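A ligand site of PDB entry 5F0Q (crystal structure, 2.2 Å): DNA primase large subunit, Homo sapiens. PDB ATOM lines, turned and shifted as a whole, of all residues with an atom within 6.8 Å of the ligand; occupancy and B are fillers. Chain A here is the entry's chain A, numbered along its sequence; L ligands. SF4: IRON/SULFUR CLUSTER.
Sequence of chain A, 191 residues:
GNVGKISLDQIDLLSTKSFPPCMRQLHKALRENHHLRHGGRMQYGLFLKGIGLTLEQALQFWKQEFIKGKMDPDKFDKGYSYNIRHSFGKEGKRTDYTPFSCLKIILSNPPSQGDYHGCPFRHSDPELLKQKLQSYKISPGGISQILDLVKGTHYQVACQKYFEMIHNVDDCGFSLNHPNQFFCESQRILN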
ATOM      1  N   PRO A  20       7.237  -1.614   7.662  1.00  0.00           N
ATOM      2  CA  PRO A  20       8.538  -1.482   7.004  1.00  0.00           C
ATOM      3  C   PRO A  20       8.278  -0.910   5.592  1.00  0.00           C
ATOM      4  O   PRO A  20       7.132  -0.909   5.125  1.00  0.00           O
ATOM      5  CB  PRO A  20       9.073  -2.919   6.987  1.00  0.00           C
ATOM      6  CG  PRO A  20       7.823  -3.731   6.980  1.00  0.00           C
ATOM      7  CD  PRO A  20       6.952  -3.020   7.970  1.00  0.00           C
ATOM      8  N   PRO A  21       9.309  -0.432   4.897  1.00  0.00           N
ATOM      9  CA  PRO A  21       9.048   0.124   3.562  1.00  0.00           C
ATOM     10  C   PRO A  21       8.156  -0.672   2.586  1.00  0.00           C
ATOM     11  O   PRO A  21       7.292  -0.084   1.921  1.00  0.00           O
ATOM     12  CB  PRO A  21      10.453   0.389   3.008  1.00  0.00           C
ATOM     13  CG  PRO A  21      11.384  -0.337   3.942  1.00  0.00           C
ATOM     14  CD  PRO A  21      10.721  -0.275   5.263  1.00  0.00           C
ATOM     15  N   CYS A  22       8.325  -1.976   2.504  1.00  0.00           N
ATOM     16  CA  CYS A  22       7.510  -2.768   1.592  1.00  0.00           C
ATOM     17  C   CYS A  22       6.025  -2.611   1.892  1.00  0.00           C
ATOM     18  O   CYS A  22       5.246  -2.196   1.024  1.00  0.00           O
ATOM     19  CB  CYS A  22       7.891  -4.241   1.660  1.00  0.00           C
ATOM     20  SG  CYS A  22       7.638  -5.028   3.267  1.00  0.00           S
ATOM     21  N   MET A  23       5.627  -2.930   3.122  1.00  0.00           N
ATOM     22  CA  MET A  23       4.224  -2.830   3.508  1.00  0.00           C
ATOM     23  C   MET A  23       3.694  -1.412   3.402  1.00  0.00           C
ATOM     24  O   MET A  23       2.518  -1.185   3.066  1.00  0.00           O
ATOM     25  CB  MET A  23       4.031  -3.375   4.923  1.00  0.00           C
ATOM     26  CG  MET A  23       4.556  -4.789   5.126  1.00  0.00           C
ATOM     27  SD  MET A  23       3.874  -5.977   3.943  1.00  0.00           S
ATOM     28  CE  MET A  23       5.027  -7.345   4.130  1.00  0.00           C
ATOM     29  N   GLN A  43       1.154 -10.569  -0.101  1.00  0.00           N
ATOM     30  CA  GLN A  43       2.140 -10.016   0.817  1.00  0.00           C
ATOM     31  C   GLN A  43       1.519  -9.119   1.889  1.00  0.00           C
ATOM     32  O   GLN A  43       1.812  -9.275   3.078  1.00  0.00           O
ATOM     33  CB  GLN A  43       3.191  -9.224   0.032  1.00  0.00           C
ATOM     34  CG  GLN A  43       4.352  -8.721   0.867  1.00  0.00           C
ATOM     35  CD  GLN A  43       5.486  -8.178   0.027  1.00  0.00           C
ATOM     36  OE1 GLN A  43       5.748  -8.654  -1.076  1.00  0.00           O
ATOM     37  NE2 GLN A  43       6.182  -7.181   0.539  1.00  0.00           N
ATOM     38  N   SER A 101       8.227 -13.998   4.842  1.00  0.00           N
ATOM     39  CA  SER A 101       9.503 -13.602   5.414  1.00  0.00           C
ATOM     40  C   SER A 101      10.268 -12.751   4.400  1.00  0.00           C
ATOM     41  O   SER A 101       9.940 -12.725   3.223  1.00  0.00           O
ATOM     42  CB  SER A 101      10.339 -14.828   5.731  1.00  0.00           C
ATOM     43  OG  SER A 101      10.749 -15.440   4.525  1.00  0.00           O
ATOM     44  N   CYS A 102      11.296 -12.067   4.857  1.00  0.00           N
ATOM     45  CA  CYS A 102      12.066 -11.236   3.957  1.00  0.00           C
ATOM     46  C   CYS A 102      12.713 -12.004   2.820  1.00  0.00           C
ATOM     47  O   CYS A 102      12.564 -11.649   1.656  1.00  0.00           O
ATOM     48  CB  CYS A 102      13.144 -10.484   4.713  1.00  0.00           C
ATOM     49  SG  CYS A 102      12.475  -9.312   5.882  1.00  0.00           S
ATOM     50  N   LEU A 103      13.447 -13.055   3.161  1.00  0.00           N
ATOM     51  CA  LEU A 103      14.137 -13.836   2.160  1.00  0.00           C
ATOM     52  C   LEU A 103      13.209 -14.262   1.034  1.00  0.00           C
ATOM     53  O   LEU A 103      13.587 -14.280  -0.142  1.00  0.00           O
ATOM     54  CB  LEU A 103      14.801 -15.048   2.824  1.00  0.00           C
ATOM     55  CG  LEU A 103      15.803 -15.802   1.939  1.00  0.00           C
ATOM     56  CD1 LEU A 103      16.876 -14.841   1.426  1.00  0.00           C
ATOM     57  CD2 LEU A 103      16.431 -16.952   2.726  1.00  0.00           C
ATOM     58  N   ILE A 105      10.309 -12.697   0.155  1.00  0.00           N
ATOM     59  CA  ILE A 105       9.906 -11.516  -0.581  1.00  0.00           C
ATOM     60  C   ILE A 105      11.004 -11.019  -1.505  1.00  0.00           C
ATOM     61  O   ILE A 105      10.746 -10.528  -2.598  1.00  0.00           O
ATOM     62  CB  ILE A 105       9.508 -10.383   0.382  1.00  0.00           C
ATOM     63  CG1 ILE A 105       8.304 -10.837   1.228  1.00  0.00           C
ATOM     64  CG2 ILE A 105       9.224  -9.112  -0.399  1.00  0.00           C
ATOM     65  CD1 ILE A 105       8.079 -10.025   2.486  1.00  0.00           C
ATOM     66  N   ILE A 106      12.247 -11.160  -1.047  1.00  0.00           N
ATOM     67  CA  ILE A 106      13.383 -10.698  -1.804  1.00  0.00           C
ATOM     68  C   ILE A 106      13.817 -11.615  -2.948  1.00  0.00           C
ATOM     69  O   ILE A 106      14.145 -11.125  -4.031  1.00  0.00           O
ATOM     70  CB  ILE A 106      14.567 -10.475  -0.841  1.00  0.00           C
ATOM     71  CG1 ILE A 106      14.297  -9.210  -0.014  1.00  0.00           C
ATOM     72  CG2 ILE A 106      15.868 -10.383  -1.621  1.00  0.00           C
ATOM     73  CD1 ILE A 106      15.286  -8.983   1.127  1.00  0.00           C
ATOM     74  N   GLY A 118       6.962  -7.025  -3.120  1.00  0.00           N
ATOM     75  CA  GLY A 118       8.406  -7.170  -3.216  1.00  0.00           C
ATOM     76  C   GLY A 118       9.116  -6.363  -2.139  1.00  0.00           C
ATOM     77  O   GLY A 118       8.480  -5.835  -1.236  1.00  0.00           O
ATOM     78  N   CYS A 119      10.443  -6.277  -2.243  1.00  0.00           N
ATOM     79  CA  CYS A 119      11.283  -5.553  -1.286  1.00  0.00           C
ATOM     80  C   CYS A 119      11.870  -4.327  -1.996  1.00  0.00           C
ATOM     81  O   CYS A 119      12.705  -4.477  -2.892  1.00  0.00           O
ATOM     82  CB  CYS A 119      12.420  -6.467  -0.809  1.00  0.00           C
ATOM     83  SG  CYS A 119      13.764  -5.671   0.127  1.00  0.00           S
ATOM     84  N   PRO A 120      11.434  -3.115  -1.625  1.00  0.00           N
ATOM     85  CA  PRO A 120      11.928  -1.879  -2.243  1.00  0.00           C
ATOM     86  C   PRO A 120      13.443  -1.821  -2.377  1.00  0.00           C
ATOM     87  O   PRO A 120      13.971  -1.409  -3.406  1.00  0.00           O
ATOM     88  CB  PRO A 120      11.388  -0.791  -1.329  1.00  0.00           C
ATOM     89  CG  PRO A 120      10.098  -1.372  -0.865  1.00  0.00           C
ATOM     90  CD  PRO A 120      10.475  -2.799  -0.548  1.00  0.00           C
ATOM     91  N   PHE A 121      14.136  -2.230  -1.321  1.00  0.00           N
ATOM     92  CA  PHE A 121      15.590  -2.208  -1.288  1.00  0.00           C
ATOM     93  C   PHE A 121      16.184  -3.148  -2.332  1.00  0.00           C
ATOM     94  O   PHE A 121      17.360  -3.037  -2.690  1.00  0.00           O
ATOM     95  CB  PHE A 121      16.087  -2.589   0.115  1.00  0.00           C
ATOM     96  CG  PHE A 121      15.711  -1.586   1.165  1.00  0.00           C
ATOM     97  CD1 PHE A 121      16.373  -0.367   1.258  1.00  0.00           C
ATOM     98  CD2 PHE A 121      14.658  -1.843   2.028  1.00  0.00           C
ATOM     99  CE1 PHE A 121      15.977   0.590   2.196  1.00  0.00           C
ATOM    100  CE2 PHE A 121      14.260  -0.890   2.980  1.00  0.00           C
ATOM    101  CZ  PHE A 121      14.911   0.327   3.062  1.00  0.00           C
ATOM    102  N   ARG A 122      15.365  -4.062  -2.833  1.00  0.00           N
ATOM    103  CA  ARG A 122      15.815  -5.024  -3.816  1.00  0.00           C
ATOM    104  C   ARG A 122      15.171  -4.862  -5.183  1.00  0.00           C
ATOM    105  O   ARG A 122      15.815  -5.097  -6.199  1.00  0.00           O
ATOM    106  CB  ARG A 122      15.564  -6.444  -3.291  1.00  0.00           C
ATOM    107  CG  ARG A 122      15.715  -7.521  -4.337  1.00  0.00           C
ATOM    108  CD  ARG A 122      17.077  -7.439  -4.992  1.00  0.00           C
ATOM    109  NE  ARG A 122      17.039  -7.877  -6.375  1.00  0.00           N
ATOM    110  CZ  ARG A 122      16.775  -9.115  -6.766  1.00  0.00           C
ATOM    111  NH1 ARG A 122      16.525 -10.069  -5.879  1.00  0.00           N
ATOM    112  NH2 ARG A 122      16.755  -9.399  -8.069  1.00  0.00           N
ATOM    113  N   TYR A 155      20.164  -5.997   1.538  1.00  0.00           N
ATOM    114  CA  TYR A 155      18.846  -5.377   1.568  1.00  0.00           C
ATOM    115  C   TYR A 155      18.218  -5.284   2.947  1.00  0.00           C
ATOM    116  O   TYR A 155      17.702  -4.233   3.322  1.00  0.00           O
ATOM    117  CB  TYR A 155      17.911  -6.149   0.628  1.00  0.00           C
ATOM    118  CG  TYR A 155      18.508  -6.363  -0.737  1.00  0.00           C
ATOM    119  CD1 TYR A 155      18.735  -5.284  -1.595  1.00  0.00           C
ATOM    120  CD2 TYR A 155      18.882  -7.637  -1.172  1.00  0.00           C
ATOM    121  CE1 TYR A 155      19.323  -5.474  -2.844  1.00  0.00           C
ATOM    122  CE2 TYR A 155      19.470  -7.841  -2.417  1.00  0.00           C
ATOM    123  CZ  TYR A 155      19.692  -6.755  -3.252  1.00  0.00           C
ATOM    124  OH  TYR A 155      20.293  -6.938  -4.474  1.00  0.00           O
ATOM    125  N   GLN A 156      18.258  -6.384   3.693  1.00  0.00           N
ATOM    126  CA  GLN A 156      17.678  -6.431   5.042  1.00  0.00           C
ATOM    127  C   GLN A 156      18.367  -5.463   5.981  1.00  0.00           C
ATOM    128  O   GLN A 156      17.718  -4.848   6.832  1.00  0.00           O
ATOM    129  CB  GLN A 156      17.773  -7.838   5.601  1.00  0.00           C
ATOM    130  CG  GLN A 156      16.672  -8.755   5.100  1.00  0.00           C
ATOM    131  CD  GLN A 156      17.196 -10.136   4.779  1.00  0.00           C
ATOM    132  OE1 GLN A 156      17.820 -10.337   3.733  1.00  0.00           O
ATOM    133  NE2 GLN A 156      16.960 -11.080   5.679  1.00  0.00           N
ATOM    134  N   VAL A 157      19.686  -5.335   5.843  1.00  0.00           N
ATOM    135  CA  VAL A 157      20.469  -4.430   6.662  1.00  0.00           C
ATOM    136  C   VAL A 157      20.084  -2.987   6.318  1.00  0.00           C
ATOM    137  O   VAL A 157      19.903  -2.166   7.209  1.00  0.00           O
ATOM    138  CB  VAL A 157      21.975  -4.622   6.393  1.00  0.00           C
ATOM    139  CG1 VAL A 157      22.774  -3.606   7.184  1.00  0.00           C
ATOM    140  CG2 VAL A 157      22.378  -6.035   6.762  1.00  0.00           C
ATOM    141  N   ALA A 158      19.961  -2.712   5.026  1.00  0.00           N
ATOM    142  CA  ALA A 158      19.568  -1.378   4.555  1.00  0.00           C
ATOM    143  C   ALA A 158      18.227  -1.009   5.173  1.00  0.00           C
ATOM    144  O   ALA A 158      17.939   0.163   5.445  1.00  0.00           O
ATOM    145  CB  ALA A 158      19.464  -1.372   3.030  1.00  0.00           C
ATOM    146  N   CYS A 159      17.394  -2.023   5.405  1.00  0.00           N
ATOM    147  CA  CYS A 159      16.075  -1.797   5.980  1.00  0.00           C
ATOM    148  C   CYS A 159      16.218  -1.529   7.460  1.00  0.00           C
ATOM    149  O   CYS A 159      15.513  -0.674   8.011  1.00  0.00           O
ATOM    150  CB  CYS A 159      15.184  -3.012   5.750  1.00  0.00           C
ATOM    151  SG  CYS A 159      13.507  -2.766   6.355  1.00  0.00           S
ATOM    152  N   GLN A 160      17.113  -2.257   8.121  1.00  0.00           N
ATOM    153  CA  GLN A 160      17.335  -2.050   9.537  1.00  0.00           C
ATOM    154  C   GLN A 160      17.792  -0.594   9.647  1.00  0.00           C
ATOM    155  O   GLN A 160      17.341   0.145  10.540  1.00  0.00           O
ATOM    156  CB  GLN A 160      18.420  -2.998  10.057  1.00  0.00           C
ATOM    157  CG  GLN A 160      18.001  -4.474  10.037  1.00  0.00           C
ATOM    158  CD  GLN A 160      19.083  -5.411  10.566  1.00  0.00           C
ATOM    159  OE1 GLN A 160      19.002  -5.904  11.687  1.00  0.00           O
ATOM    160  NE2 GLN A 160      20.108  -5.645   9.759  1.00  0.00           N
ATOM    161  N   LEU A 176      17.025  -8.194  11.263  1.00  0.00           N
ATOM    162  CA  LEU A 176      15.769  -8.251  10.534  1.00  0.00           C
ATOM    163  C   LEU A 176      15.653  -9.360   9.512  1.00  0.00           C
ATOM    164  O   LEU A 176      16.534  -9.545   8.673  1.00  0.00           O
ATOM    165  CB  LEU A 176      15.539  -6.930   9.796  1.00  0.00           C
ATOM    166  CG  LEU A 176      14.186  -6.859   9.109  1.00  0.00           C
ATOM    167  CD1 LEU A 176      13.110  -6.784  10.169  1.00  0.00           C
ATOM    168  CD2 LEU A 176      14.126  -5.654   8.211  1.00  0.00           C
ATOM    169  N   ASN A 177      14.563 -10.099   9.579  1.00  0.00           N
ATOM    170  CA  ASN A 177      14.357 -11.138   8.577  1.00  0.00           C
ATOM    171  C   ASN A 177      12.881 -11.473   8.368  1.00  0.00           C
ATOM    172  O   ASN A 177      12.538 -12.499   7.792  1.00  0.00           O
ATOM    173  CB  ASN A 177      15.160 -12.392   8.925  1.00  0.00           C
ATOM    174  CG  ASN A 177      14.959 -12.812  10.344  1.00  0.00           C
ATOM    175  OD1 ASN A 177      13.828 -12.919  10.820  1.00  0.00           O
ATOM    176  ND2 ASN A 177      16.063 -13.066  11.039  1.00  0.00           N
ATOM    177  N   HIS A 178      12.016 -10.581   8.815  1.00  0.00           N
ATOM    178  CA  HIS A 178      10.592 -10.757   8.620  1.00  0.00           C
ATOM    179  C   HIS A 178       9.879  -9.429   8.861  1.00  0.00           C
ATOM    180  O   HIS A 178      10.090  -8.780   9.885  1.00  0.00           O
ATOM    181  CB  HIS A 178      10.071 -11.847   9.555  1.00  0.00           C
ATOM    182  CG  HIS A 178       8.715 -12.365   9.182  1.00  0.00           C
ATOM    183  ND1 HIS A 178       7.588 -11.564   9.201  1.00  0.00           N
ATOM    184  CD2 HIS A 178       8.298 -13.601   8.834  1.00  0.00           C
ATOM    185  CE1 HIS A 178       6.534 -12.292   8.877  1.00  0.00           C
ATOM    186  NE2 HIS A 178       6.935 -13.538   8.654  1.00  0.00           N
ATOM    187  N   PRO A 179       9.050  -8.988   7.904  1.00  0.00           N
ATOM    188  CA  PRO A 179       8.304  -7.726   8.011  1.00  0.00           C
ATOM    189  C   PRO A 179       7.541  -7.487   9.312  1.00  0.00           C
ATOM    190  O   PRO A 179       7.543  -6.383   9.833  1.00  0.00           O
ATOM    191  CB  PRO A 179       7.378  -7.777   6.786  1.00  0.00           C
ATOM    192  CG  PRO A 179       8.210  -8.511   5.791  1.00  0.00           C
ATOM    193  CD  PRO A 179       8.772  -9.649   6.622  1.00  0.00           C
ATOM    194  N   ASN A 180       6.854  -8.505   9.819  1.00  0.00           N
ATOM    195  CA  ASN A 180       6.101  -8.316  11.042  1.00  0.00           C
ATOM    196  C   ASN A 180       7.017  -8.159  12.256  1.00  0.00           C
ATOM    197  O   ASN A 180       6.594  -7.718  13.317  1.00  0.00           O
ATOM    198  CB  ASN A 180       5.139  -9.477  11.252  1.00  0.00           C
ATOM    199  CG  ASN A 180       4.054  -9.519  10.197  1.00  0.00           C
ATOM    200  OD1 ASN A 180       4.281  -9.983   9.085  1.00  0.00           O
ATOM    201  ND2 ASN A 180       2.869  -9.010  10.544  1.00  0.00           N
ATOM    202  N   PHE A 182       9.738  -6.284  12.024  1.00  0.00           N
ATOM    203  CA  PHE A 182      10.023  -4.852  11.915  1.00  0.00           C
ATOM    204  C   PHE A 182       8.862  -4.086  12.557  1.00  0.00           C
ATOM    205  O   PHE A 182       9.071  -3.065  13.199  1.00  0.00           O
ATOM    206  CB  PHE A 182      10.177  -4.470  10.443  1.00  0.00           C
ATOM    207  CG  PHE A 182      10.434  -2.986  10.203  1.00  0.00           C
ATOM    208  CD1 PHE A 182      11.631  -2.562   9.652  1.00  0.00           C
ATOM    209  CD2 PHE A 182       9.435  -2.041  10.422  1.00  0.00           C
ATOM    210  CE1 PHE A 182      11.840  -1.227   9.298  1.00  0.00           C
ATOM    211  CE2 PHE A 182       9.617  -0.695  10.081  1.00  0.00           C
ATOM    212  CZ  PHE A 182      10.818  -0.291   9.511  1.00  0.00           C
HETATM  213 FE1  SF4 L   1      12.268  -7.355   4.632  1.00  0.00          FE
HETATM  214 FE2  SF4 L   1      12.642  -5.683   2.342  1.00  0.00          FE
HETATM  215 FE3  SF4 L   1      12.533  -4.386   4.995  1.00  0.00          FE
HETATM  216 FE4  SF4 L   1       9.844  -5.612   3.659  1.00  0.00          FE
HETATM  217  S1  SF4 L   1      11.326  -4.143   3.191  1.00  0.00           S
HETATM  218  S2  SF4 L   1      10.950  -5.818   5.494  1.00  0.00           S
HETATM  219  S3  SF4 L   1      11.058  -7.116   2.811  1.00  0.00           S
HETATM  220  S4  SF4 L   1      13.762  -5.879   4.160  1.00  0.00           S
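A sulfur (S1) of the ligand sits close to the backbone NH (N) of Cys 22 (3.8 Å). The side-chain sulfur of Cys 22 is bound to an iron atom (FE4) of the ligand (2.3 Å). An iron atom (FE3) of the ligand is bound by the side-chain sulfur (SG) of Cys 159 (2.3 Å). FE1 of the ligand is bound by SG of Cys 102, 2.3 Å away. SG of Cys 119 binds FE2 of the ligand.
Residues that only touch the ligand: Pro 20, Pro 21, Leu 176 and Pro 179. Hydrophobic or aromatic side chains that line the ligand: Pro 20, Pro 21, Leu 176 and Pro 179. Of the 27 residues printed, 8 come within 4 Å of the ligand.
The side-chain amide nitrogen (NE2) of Gln 43 sits close to the side-chain sulfur (SG) of Cys 22, 3.8 Å away. The backbone NH (N) of His 178 lies close to the side-chain sulfur (SG) of Cys 102 (3.2 Å). The backbone NH of Cys 102 sits at hydrogen-bond distance from the backbone carbonyl oxygen of Asn 177 (3.2 Å). The side-chain sulfur (SG) of Cys 119 lies close to the backbone NH (N) of Phe 121 (3.8 Å). The side-chain sulfur of Cys 119 sits close to the backbone NH of Arg 122 (3.7 Å). NE2 of Gln 156 is in hydrogen-bond range of O of Leu 176. The backbone NH (N) of Leu 176 sits at hydrogen-bond distance from the side-chain amide oxygen (OE1) of Gln 160 (3.1 Å).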
